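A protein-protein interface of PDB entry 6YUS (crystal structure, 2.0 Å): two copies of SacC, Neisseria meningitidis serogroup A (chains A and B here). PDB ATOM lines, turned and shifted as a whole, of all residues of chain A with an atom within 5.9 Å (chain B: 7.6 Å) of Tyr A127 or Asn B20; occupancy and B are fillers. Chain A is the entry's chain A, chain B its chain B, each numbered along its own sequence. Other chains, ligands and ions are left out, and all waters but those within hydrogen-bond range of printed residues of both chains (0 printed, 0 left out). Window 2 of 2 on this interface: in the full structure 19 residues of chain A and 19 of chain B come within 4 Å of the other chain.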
ATOM      1  N   ASN A  87     -18.062  11.195 -11.060  1.00  0.00           N
ATOM      2  CA  ASN A  87     -17.236  12.071 -11.892  1.00  0.00           C
ATOM      3  C   ASN A  87     -16.061  11.343 -12.540  1.00  0.00           C
ATOM      4  O   ASN A  87     -15.244  12.002 -13.192  1.00  0.00           O
ATOM      5  CB  ASN A  87     -16.669  13.232 -11.073  1.00  0.00           C
ATOM      6  CG  ASN A  87     -17.737  14.213 -10.598  1.00  0.00           C
ATOM      7  OD1 ASN A  87     -18.825  14.283 -11.143  1.00  0.00           O
ATOM      8  ND2 ASN A  87     -17.408  14.985  -9.586  1.00  0.00           N
ATOM      9  N   LEU A  90     -15.370  12.302 -16.307  1.00  0.00           N
ATOM     10  CA  LEU A  90     -14.979  13.712 -16.355  1.00  0.00           C
ATOM     11  C   LEU A  90     -13.592  13.932 -15.773  1.00  0.00           C
ATOM     12  O   LEU A  90     -12.858  14.824 -16.211  1.00  0.00           O
ATOM     13  CB  LEU A  90     -15.985  14.572 -15.578  1.00  0.00           C
ATOM     14  CG  LEU A  90     -17.433  14.440 -16.046  1.00  0.00           C
ATOM     15  CD1 LEU A  90     -18.360  14.986 -14.939  1.00  0.00           C
ATOM     16  CD2 LEU A  90     -17.654  15.189 -17.364  1.00  0.00           C
ATOM     17  N   GLN A  91     -13.236  13.166 -14.746  1.00  0.00           N
ATOM     18  CA  GLN A  91     -11.924  13.319 -14.129  1.00  0.00           C
ATOM     19  C   GLN A  91     -10.804  12.908 -15.083  1.00  0.00           C
ATOM     20  O   GLN A  91      -9.732  13.528 -15.109  1.00  0.00           O
ATOM     21  CB  GLN A  91     -11.892  12.487 -12.852  1.00  0.00           C
ATOM     22  CG  GLN A  91     -10.567  12.361 -12.208  1.00  0.00           C
ATOM     23  CD  GLN A  91     -10.647  11.418 -11.039  1.00  0.00           C
ATOM     24  OE1 GLN A  91     -11.697  11.350 -10.396  1.00  0.00           O
ATOM     25  NE2 GLN A  91      -9.557  10.654 -10.765  1.00  0.00           N
ATOM     26  N   THR A  92     -11.027  11.855 -15.864  1.00  0.00           N
ATOM     27  CA  THR A  92     -10.062  11.454 -16.877  1.00  0.00           C
ATOM     28  C   THR A  92      -9.915  12.521 -17.957  1.00  0.00           C
ATOM     29  O   THR A  92      -8.796  12.857 -18.375  1.00  0.00           O
ATOM     30  CB  THR A  92     -10.492  10.119 -17.487  1.00  0.00           C
ATOM     31  OG1 THR A  92     -10.310   9.083 -16.513  1.00  0.00           O
ATOM     32  CG2 THR A  92      -9.631   9.794 -18.707  1.00  0.00           C
ATOM     33  N   HIS A  94     -10.416  15.682 -17.646  1.00  0.00           N
ATOM     34  CA  HIS A  94      -9.698  16.794 -17.025  1.00  0.00           C
ATOM     35  C   HIS A  94      -8.190  16.574 -17.072  1.00  0.00           C
ATOM     36  O   HIS A  94      -7.422  17.460 -17.491  1.00  0.00           O
ATOM     37  CB  HIS A  94     -10.194  16.956 -15.575  1.00  0.00           C
ATOM     38  CG  HIS A  94      -9.626  18.135 -14.858  1.00  0.00           C
ATOM     39  ND1 HIS A  94      -9.617  19.400 -15.409  1.00  0.00           N
ATOM     40  CD2 HIS A  94      -9.041  18.248 -13.638  1.00  0.00           C
ATOM     41  CE1 HIS A  94      -9.075  20.247 -14.552  1.00  0.00           C
ATOM     42  NE2 HIS A  94      -8.720  19.576 -13.468  1.00  0.00           N
ATOM     43  N   CYS A  95      -7.738  15.388 -16.638  1.00  0.00           N
ATOM     44  CA  CYS A  95      -6.300  15.110 -16.639  1.00  0.00           C
ATOM     45  C   CYS A  95      -5.724  15.227 -18.036  1.00  0.00           C
ATOM     46  O   CYS A  95      -4.639  15.788 -18.233  1.00  0.00           O
ATOM     47  CB  CYS A  95      -6.011  13.715 -16.090  1.00  0.00           C
ATOM     48  SG  CYS A  95      -6.453  13.541 -14.353  1.00  0.00           S
ATOM     49  N   GLN A 105      -6.025  28.304 -18.731  1.00  0.00           N
ATOM     50  CA  GLN A 105      -7.419  27.881 -18.625  1.00  0.00           C
ATOM     51  C   GLN A 105      -8.346  28.884 -19.314  1.00  0.00           C
ATOM     52  O   GLN A 105      -9.334  28.503 -19.965  1.00  0.00           O
ATOM     53  CB  GLN A 105      -7.753  27.715 -17.134  1.00  0.00           C
ATOM     54  CG  GLN A 105      -8.978  26.870 -16.807  1.00  0.00           C
ATOM     55  CD  GLN A 105      -8.697  25.370 -16.854  1.00  0.00           C
ATOM     56  OE1 GLN A 105      -7.717  24.935 -17.469  1.00  0.00           O
ATOM     57  NE2 GLN A 105      -9.572  24.567 -16.215  1.00  0.00           N
ATOM     58  N   LEU A 122     -20.775  19.948 -17.659  1.00  0.00           N
ATOM     59  CA  LEU A 122     -20.343  19.117 -16.546  1.00  0.00           C
ATOM     60  C   LEU A 122     -18.846  19.274 -16.296  1.00  0.00           C
ATOM     61  O   LEU A 122     -18.413  19.377 -15.141  1.00  0.00           O
ATOM     62  CB  LEU A 122     -20.699  17.645 -16.806  1.00  0.00           C
ATOM     63  CG  LEU A 122     -22.175  17.263 -16.908  1.00  0.00           C
ATOM     64  CD1 LEU A 122     -22.322  15.766 -17.293  1.00  0.00           C
ATOM     65  CD2 LEU A 122     -22.915  17.590 -15.593  1.00  0.00           C
ATOM     66  N   LEU A 123     -18.034  19.302 -17.367  1.00  0.00           N
ATOM     67  CA  LEU A 123     -16.578  19.422 -17.175  1.00  0.00           C
ATOM     68  C   LEU A 123     -16.214  20.795 -16.650  1.00  0.00           C
ATOM     69  O   LEU A 123     -15.454  20.932 -15.671  1.00  0.00           O
ATOM     70  CB  LEU A 123     -15.836  19.182 -18.479  1.00  0.00           C
ATOM     71  CG  LEU A 123     -14.315  19.195 -18.255  1.00  0.00           C
ATOM     72  CD1 LEU A 123     -13.907  17.893 -17.580  1.00  0.00           C
ATOM     73  CD2 LEU A 123     -13.522  19.410 -19.547  1.00  0.00           C
ATOM     74  N   GLY A 124     -16.758  21.827 -17.300  1.00  0.00           N
ATOM     75  CA  GLY A 124     -16.362  23.184 -16.986  1.00  0.00           C
ATOM     76  C   GLY A 124     -16.778  23.604 -15.601  1.00  0.00           C
ATOM     77  O   GLY A 124     -16.025  24.292 -14.905  1.00  0.00           O
ATOM     78  N   LEU A 125     -17.982  23.200 -15.183  1.00  0.00           N
ATOM     79  CA  LEU A 125     -18.479  23.551 -13.855  1.00  0.00           C
ATOM     80  C   LEU A 125     -17.821  22.715 -12.769  1.00  0.00           C
ATOM     81  O   LEU A 125     -17.777  23.139 -11.607  1.00  0.00           O
ATOM     82  CB  LEU A 125     -19.993  23.327 -13.774  1.00  0.00           C
ATOM     83  CG  LEU A 125     -20.886  24.184 -14.672  1.00  0.00           C
ATOM     84  CD1 LEU A 125     -22.347  23.719 -14.553  1.00  0.00           C
ATOM     85  CD2 LEU A 125     -20.747  25.640 -14.298  1.00  0.00           C
ATOM     86  N   THR A 126     -17.381  21.499 -13.099  1.00  0.00           N
ATOM     87  CA  THR A 126     -16.707  20.697 -12.077  1.00  0.00           C
ATOM     88  C   THR A 126     -15.284  21.191 -11.838  1.00  0.00           C
ATOM     89  O   THR A 126     -14.828  21.243 -10.695  1.00  0.00           O
ATOM     90  CB  THR A 126     -16.693  19.210 -12.464  1.00  0.00           C
ATOM     91  OG1 THR A 126     -18.042  18.758 -12.655  1.00  0.00           O
ATOM     92  CG2 THR A 126     -16.052  18.354 -11.306  1.00  0.00           C
ATOM     93  N   TYR A 127     -14.558  21.556 -12.897  1.00  0.00           N
ATOM     94  CA  TYR A 127     -13.130  21.831 -12.770  1.00  0.00           C
ATOM     95  C   TYR A 127     -12.770  23.249 -13.171  1.00  0.00           C
ATOM     96  O   TYR A 127     -11.594  23.524 -13.402  1.00  0.00           O
ATOM     97  CB  TYR A 127     -12.320  20.827 -13.608  1.00  0.00           C
ATOM     98  CG  TYR A 127     -12.501  19.396 -13.128  1.00  0.00           C
ATOM     99  CD1 TYR A 127     -11.837  18.922 -11.964  1.00  0.00           C
ATOM    100  CD2 TYR A 127     -13.312  18.535 -13.810  1.00  0.00           C
ATOM    101  CE1 TYR A 127     -12.010  17.590 -11.522  1.00  0.00           C
ATOM    102  CE2 TYR A 127     -13.493  17.231 -13.389  1.00  0.00           C
ATOM    103  CZ  TYR A 127     -12.858  16.776 -12.254  1.00  0.00           C
ATOM    104  OH  TYR A 127     -13.104  15.489 -11.878  1.00  0.00           O
ATOM    105  N   ASN A 128     -13.747  24.152 -13.280  1.00  0.00           N
ATOM    106  CA  ASN A 128     -13.468  25.576 -13.426  1.00  0.00           C
ATOM    107  C   ASN A 128     -12.852  25.912 -14.790  1.00  0.00           C
ATOM    108  O   ASN A 128     -11.908  26.677 -14.885  1.00  0.00           O
ATOM    109  CB  ASN A 128     -12.573  26.088 -12.282  1.00  0.00           C
ATOM    110  CG  ASN A 128     -13.341  26.276 -10.974  1.00  0.00           C
ATOM    111  OD1 ASN A 128     -14.558  26.063 -10.911  1.00  0.00           O
ATOM    112  ND2 ASN A 128     -12.646  26.684  -9.940  1.00  0.00           N
ATOM    113  N   TYR A 129     -13.446  25.406 -15.863  1.00  0.00           N
ATOM    114  CA  TYR A 129     -13.110  25.910 -17.192  1.00  0.00           C
ATOM    115  C   TYR A 129     -14.085  27.042 -17.467  1.00  0.00           C
ATOM    116  O   TYR A 129     -15.292  26.775 -17.602  1.00  0.00           O
ATOM    117  CB  TYR A 129     -13.257  24.829 -18.254  1.00  0.00           C
ATOM    118  CG  TYR A 129     -12.281  23.700 -18.131  1.00  0.00           C
ATOM    119  CD1 TYR A 129     -12.503  22.657 -17.230  1.00  0.00           C
ATOM    120  CD2 TYR A 129     -11.123  23.666 -18.916  1.00  0.00           C
ATOM    121  CE1 TYR A 129     -11.581  21.609 -17.103  1.00  0.00           C
ATOM    122  CE2 TYR A 129     -10.216  22.622 -18.809  1.00  0.00           C
ATOM    123  CZ  TYR A 129     -10.448  21.596 -17.889  1.00  0.00           C
ATOM    124  OH  TYR A 129      -9.549  20.543 -17.759  1.00  0.00           O
ATOM    125  N   LEU B   5      -0.146  23.750 -13.081  1.00  0.00           N
ATOM    126  CA  LEU B   5      -0.458  22.894 -11.949  1.00  0.00           C
ATOM    127  C   LEU B   5       0.555  23.028 -10.826  1.00  0.00           C
ATOM    128  O   LEU B   5       0.426  22.336  -9.808  1.00  0.00           O
ATOM    129  CB  LEU B   5      -0.514  21.437 -12.404  1.00  0.00           C
ATOM    130  CG  LEU B   5      -1.522  21.209 -13.536  1.00  0.00           C
ATOM    131  CD1 LEU B   5      -1.328  19.805 -14.049  1.00  0.00           C
ATOM    132  CD2 LEU B   5      -2.960  21.450 -13.015  1.00  0.00           C
ATOM    133  N   GLU B  18       0.330  19.641  -8.750  1.00  0.00           N
ATOM    134  CA  GLU B  18      -0.834  18.990  -8.175  1.00  0.00           C
ATOM    135  C   GLU B  18      -1.959  18.913  -9.200  1.00  0.00           C
ATOM    136  O   GLU B  18      -2.280  19.899  -9.873  1.00  0.00           O
ATOM    137  CB  GLU B  18      -1.286  19.722  -6.899  1.00  0.00           C
ATOM    138  CG  GLU B  18      -2.586  19.207  -6.304  1.00  0.00           C
ATOM    139  CD  GLU B  18      -2.909  19.807  -4.935  1.00  0.00           C
ATOM    140  OE1 GLU B  18      -2.030  19.873  -4.075  1.00  0.00           O
ATOM    141  OE2 GLU B  18      -4.052  20.171  -4.701  1.00  0.00           O
ATOM    142  N   LEU B  19      -2.592  17.747  -9.284  1.00  0.00           N
ATOM    143  CA  LEU B  19      -3.682  17.546 -10.231  1.00  0.00           C
ATOM    144  C   LEU B  19      -4.730  16.673  -9.571  1.00  0.00           C
ATOM    145  O   LEU B  19      -4.449  15.532  -9.199  1.00  0.00           O
ATOM    146  CB  LEU B  19      -3.186  16.895 -11.524  1.00  0.00           C
ATOM    147  CG  LEU B  19      -4.300  16.530 -12.524  1.00  0.00           C
ATOM    148  CD1 LEU B  19      -4.955  17.761 -13.069  1.00  0.00           C
ATOM    149  CD2 LEU B  19      -3.700  15.697 -13.674  1.00  0.00           C
ATOM    150  N   ASN B  20      -5.932  17.205  -9.416  1.00  0.00           N
ATOM    151  CA  ASN B  20      -7.011  16.444  -8.802  1.00  0.00           C
ATOM    152  C   ASN B  20      -6.655  15.941  -7.424  1.00  0.00           C
ATOM    153  O   ASN B  20      -7.010  14.813  -7.081  1.00  0.00           O
ATOM    154  CB  ASN B  20      -7.400  15.258  -9.667  1.00  0.00           C
ATOM    155  CG  ASN B  20      -8.497  15.554 -10.482  1.00  0.00           C
ATOM    156  OD1 ASN B  20      -8.338  15.749 -11.681  1.00  0.00           O
ATOM    157  ND2 ASN B  20      -9.674  15.682  -9.857  1.00  0.00           N
ATOM    158  N   GLY B  21      -5.961  16.781  -6.630  1.00  0.00           N
ATOM    159  CA  GLY B  21      -5.591  16.428  -5.279  1.00  0.00           C
ATOM    160  C   GLY B  21      -4.353  15.567  -5.185  1.00  0.00           C
ATOM    161  O   GLY B  21      -4.003  15.123  -4.090  1.00  0.00           O
ATOM    162  N   CYS B  22      -3.681  15.327  -6.289  1.00  0.00           N
ATOM    163  CA  CYS B  22      -2.578  14.376  -6.362  1.00  0.00           C
ATOM    164  C   CYS B  22      -1.303  15.179  -6.582  1.00  0.00           C
ATOM    165  O   CYS B  22      -1.141  15.806  -7.634  1.00  0.00           O
ATOM    166  CB  CYS B  22      -2.824  13.382  -7.506  1.00  0.00           C
ATOM    167  SG  CYS B  22      -1.332  12.386  -7.788  1.00  0.00           S
ATOM    168  N   ARG B  23      -0.419  15.191  -5.583  1.00  0.00           N
ATOM    169  CA  ARG B  23       0.809  15.971  -5.640  1.00  0.00           C
ATOM    170  C   ARG B  23       1.952  15.109  -6.172  1.00  0.00           C
ATOM    171  O   ARG B  23       2.124  13.974  -5.740  1.00  0.00           O
ATOM    172  CB  ARG B  23       1.174  16.497  -4.243  1.00  0.00           C
ATOM    173  CG  ARG B  23       0.161  17.484  -3.668  1.00  0.00           C
ATOM    174  CD  ARG B  23       0.349  17.580  -2.161  1.00  0.00           C
ATOM    175  NE  ARG B  23      -0.142  16.375  -1.495  1.00  0.00           N
ATOM    176  CZ  ARG B  23      -0.058  16.136  -0.193  1.00  0.00           C
ATOM    177  NH1 ARG B  23       0.511  17.023   0.615  1.00  0.00           N
ATOM    178  NH2 ARG B  23      -0.552  15.006   0.296  1.00  0.00           N
ATOM    179  N   PHE B  24       2.753  15.667  -7.080  1.00  0.00           N
ATOM    180  CA  PHE B  24       3.827  14.887  -7.674  1.00  0.00           C
ATOM    181  C   PHE B  24       4.977  15.781  -8.090  1.00  0.00           C
ATOM    182  O   PHE B  24       4.814  16.983  -8.324  1.00  0.00           O
ATOM    183  CB  PHE B  24       3.354  14.079  -8.893  1.00  0.00           C
ATOM    184  CG  PHE B  24       2.836  14.913 -10.042  1.00  0.00           C
ATOM    185  CD1 PHE B  24       1.532  15.389 -10.047  1.00  0.00           C
ATOM    186  CD2 PHE B  24       3.640  15.170 -11.135  1.00  0.00           C
ATOM    187  CE1 PHE B  24       1.023  16.110 -11.139  1.00  0.00           C
ATOM    188  CE2 PHE B  24       3.164  15.880 -12.226  1.00  0.00           C
ATOM    189  CZ  PHE B  24       1.833  16.367 -12.223  1.00  0.00           C
ATOM    190  N   LYS B  69      -4.588  13.959   0.468  1.00  0.00           N
ATOM    191  CA  LYS B  69      -4.438  15.118   1.361  1.00  0.00           C
ATOM    192  C   LYS B  69      -5.429  15.154   2.523  1.00  0.00           C
ATOM    193  O   LYS B  69      -5.517  16.176   3.227  1.00  0.00           O
ATOM    194  CB  LYS B  69      -4.588  16.418   0.570  1.00  0.00           C
ATOM    195  CG  LYS B  69      -3.566  16.568  -0.562  1.00  0.00           C
ATOM    196  CD  LYS B  69      -4.065  17.652  -1.526  1.00  0.00           C
ATOM    197  CE  LYS B  69      -4.109  18.997  -0.843  1.00  0.00           C
ATOM    198  NZ  LYS B  69      -4.233  20.099  -1.829  1.00  0.00           N
ATOM    199  N   TYR B  70      -6.180  14.087   2.736  1.00  0.00           N
ATOM    200  CA  TYR B  70      -7.189  14.021   3.774  1.00  0.00           C
ATOM    201  C   TYR B  70      -6.937  12.764   4.591  1.00  0.00           C
ATOM    202  O   TYR B  70      -6.373  11.797   4.070  1.00  0.00           O
ATOM    203  CB  TYR B  70      -8.614  14.004   3.167  1.00  0.00           C
ATOM    204  CG  TYR B  70      -8.809  13.202   1.882  1.00  0.00           C
ATOM    205  CD1 TYR B  70      -8.624  11.812   1.860  1.00  0.00           C
ATOM    206  CD2 TYR B  70      -9.227  13.822   0.699  1.00  0.00           C
ATOM    207  CE1 TYR B  70      -8.836  11.046   0.691  1.00  0.00           C
ATOM    208  CE2 TYR B  70      -9.457  13.062  -0.485  1.00  0.00           C
ATOM    209  CZ  TYR B  70      -9.255  11.673  -0.480  1.00  0.00           C
ATOM    210  OH  TYR B  70      -9.464  10.912  -1.628  1.00  0.00           O
ATOM    211  N   GLY B  88     -10.191   6.264  -7.505  1.00  0.00           N
ATOM    212  CA  GLY B  88     -10.063   7.584  -8.105  1.00  0.00           C
ATOM    213  C   GLY B  88      -8.663   8.173  -7.996  1.00  0.00           C
ATOM    214  O   GLY B  88      -8.186   8.851  -8.910  1.00  0.00           O
ATOM    215  N   TYR B  89      -7.974   7.905  -6.912  1.00  0.00           N
ATOM    216  CA  TYR B  89      -6.628   8.460  -6.768  1.00  0.00           C
ATOM    217  C   TYR B  89      -5.621   7.715  -7.652  1.00  0.00           C
ATOM    218  O   TYR B  89      -4.822   8.327  -8.366  1.00  0.00           O
ATOM    219  CB  TYR B  89      -6.222   8.429  -5.291  1.00  0.00           C
ATOM    220  CG  TYR B  89      -5.067   9.345  -4.958  1.00  0.00           C
ATOM    221  CD1 TYR B  89      -5.215  10.721  -5.058  1.00  0.00           C
ATOM    222  CD2 TYR B  89      -3.849   8.841  -4.544  1.00  0.00           C
ATOM    223  CE1 TYR B  89      -4.196  11.563  -4.760  1.00  0.00           C
ATOM    224  CE2 TYR B  89      -2.793   9.681  -4.236  1.00  0.00           C
ATOM    225  CZ  TYR B  89      -2.984  11.048  -4.362  1.00  0.00           C
ATOM    226  OH  TYR B  89      -1.974  11.926  -4.088  1.00  0.00           O
ATOM    227  N   THR B  92      -5.936   8.880 -11.187  1.00  0.00           N
ATOM    228  CA  THR B  92      -5.252  10.132 -11.480  1.00  0.00           C
ATOM    229  C   THR B  92      -3.750   9.913 -11.658  1.00  0.00           C
ATOM    230  O   THR B  92      -3.136  10.479 -12.570  1.00  0.00           O
ATOM    231  CB  THR B  92      -5.512  11.132 -10.349  1.00  0.00           C
ATOM    232  OG1 THR B  92      -6.882  11.527 -10.353  1.00  0.00           O
ATOM    233  CG2 THR B  92      -4.646  12.365 -10.504  1.00  0.00           C
ATOM    234  N   ILE B  93      -3.132   9.154 -10.750  1.00  0.00           N
ATOM    235  CA  ILE B  93      -1.709   8.810 -10.875  1.00  0.00           C
ATOM    236  C   ILE B  93      -1.433   8.185 -12.233  1.00  0.00           C
ATOM    237  O   ILE B  93      -0.447   8.518 -12.906  1.00  0.00           O
ATOM    238  CB  ILE B  93      -1.302   7.877  -9.717  1.00  0.00           C
ATOM    239  CG1 ILE B  93      -1.383   8.646  -8.393  1.00  0.00           C
ATOM    240  CG2 ILE B  93       0.141   7.332  -9.884  1.00  0.00           C
ATOM    241  CD1 ILE B  93      -1.071   7.811  -7.206  1.00  0.00           C
ATOM    242  N   ILE B  96      -1.471  10.664 -15.091  1.00  0.00           N
ATOM    243  CA  ILE B  96      -0.298  11.528 -15.032  1.00  0.00           C
ATOM    244  C   ILE B  96       0.907  10.793 -15.609  1.00  0.00           C
ATOM    245  O   ILE B  96       1.628  11.320 -16.468  1.00  0.00           O
ATOM    246  CB  ILE B  96      -0.078  11.976 -13.571  1.00  0.00           C
ATOM    247  CG1 ILE B  96      -1.226  12.873 -13.097  1.00  0.00           C
ATOM    248  CG2 ILE B  96       1.274  12.657 -13.390  1.00  0.00           C
ATOM    249  CD1 ILE B  96      -1.045  13.244 -11.643  1.00  0.00           C
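Of the printed residues of chain B, Gln A91 touches Gly B88 (2.9 Å) and Thr B92 (2.8 Å). Of the printed residues of chain B, Cys A95 touches Leu B19 and Asn B20. Tyr A127 touches one residue of chain B. Tyr A129 touches none of the printed residues of chain B. Of the printed residues of chain A, Leu B19 touches Cys A95 (3.6 Å). Cys B22 touches none of the printed residues of chain A. Of the printed residues of chain A, Thr B92 touches Gln A91. The nearest printed residue of chain A that does not touch Leu B19 is His A94 (4.2 Å).
The side-chain amide nitrogen of Gln A91 is in hydrogen-bond range of the side-chain hydroxyl of Thr B92, at 2.8 Å. O of Gly B88 lies within hydrogen-bond range of NE2 of Gln A91 (2.9 Å).
A ring nitrogen (ND1) of His A94 sits at hydrogen-bond distance from the side-chain hydroxyl (OH) of Tyr A129 (2.6 Å). The side-chain sulfur (SG) of Cys A95 lies within hydrogen-bond range of the backbone carbonyl oxygen (O) of Gln A91 (3.4 Å). O of Gly B88 lies within hydrogen-bond range of OG1 of Thr B92, 3.3 Å away.
1 position is printed for both chains. Of the 6 pairs that touch across the chains among the printed residues, none has its exchanged pair printed and touching as well.
Among the printed residues, pairs that only touch across the chains: His A94 with Asn B20 (3.3 Å), Cys A95 with Leu B19 (3.6 Å), Cys A95 with Asn B20 (3.9 Å) and Tyr A127 with Asn B20 (3.4 Å).
Of the 15 printed residues of chain B, 4 touch a printed residue of chain A. Hydrophobic or aromatic side chains of chain B within 4 Å of the printed part of chain A: Leu B19. Printed residues of chain A that touch a printed residue of chain B: Gln A91, His A94, Cys A95 and Tyr A127. Among the printed residues, no Asp or Glu carboxylate lies within 4 Å of a Lys or Arg side-chain nitrogen of the other chain.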
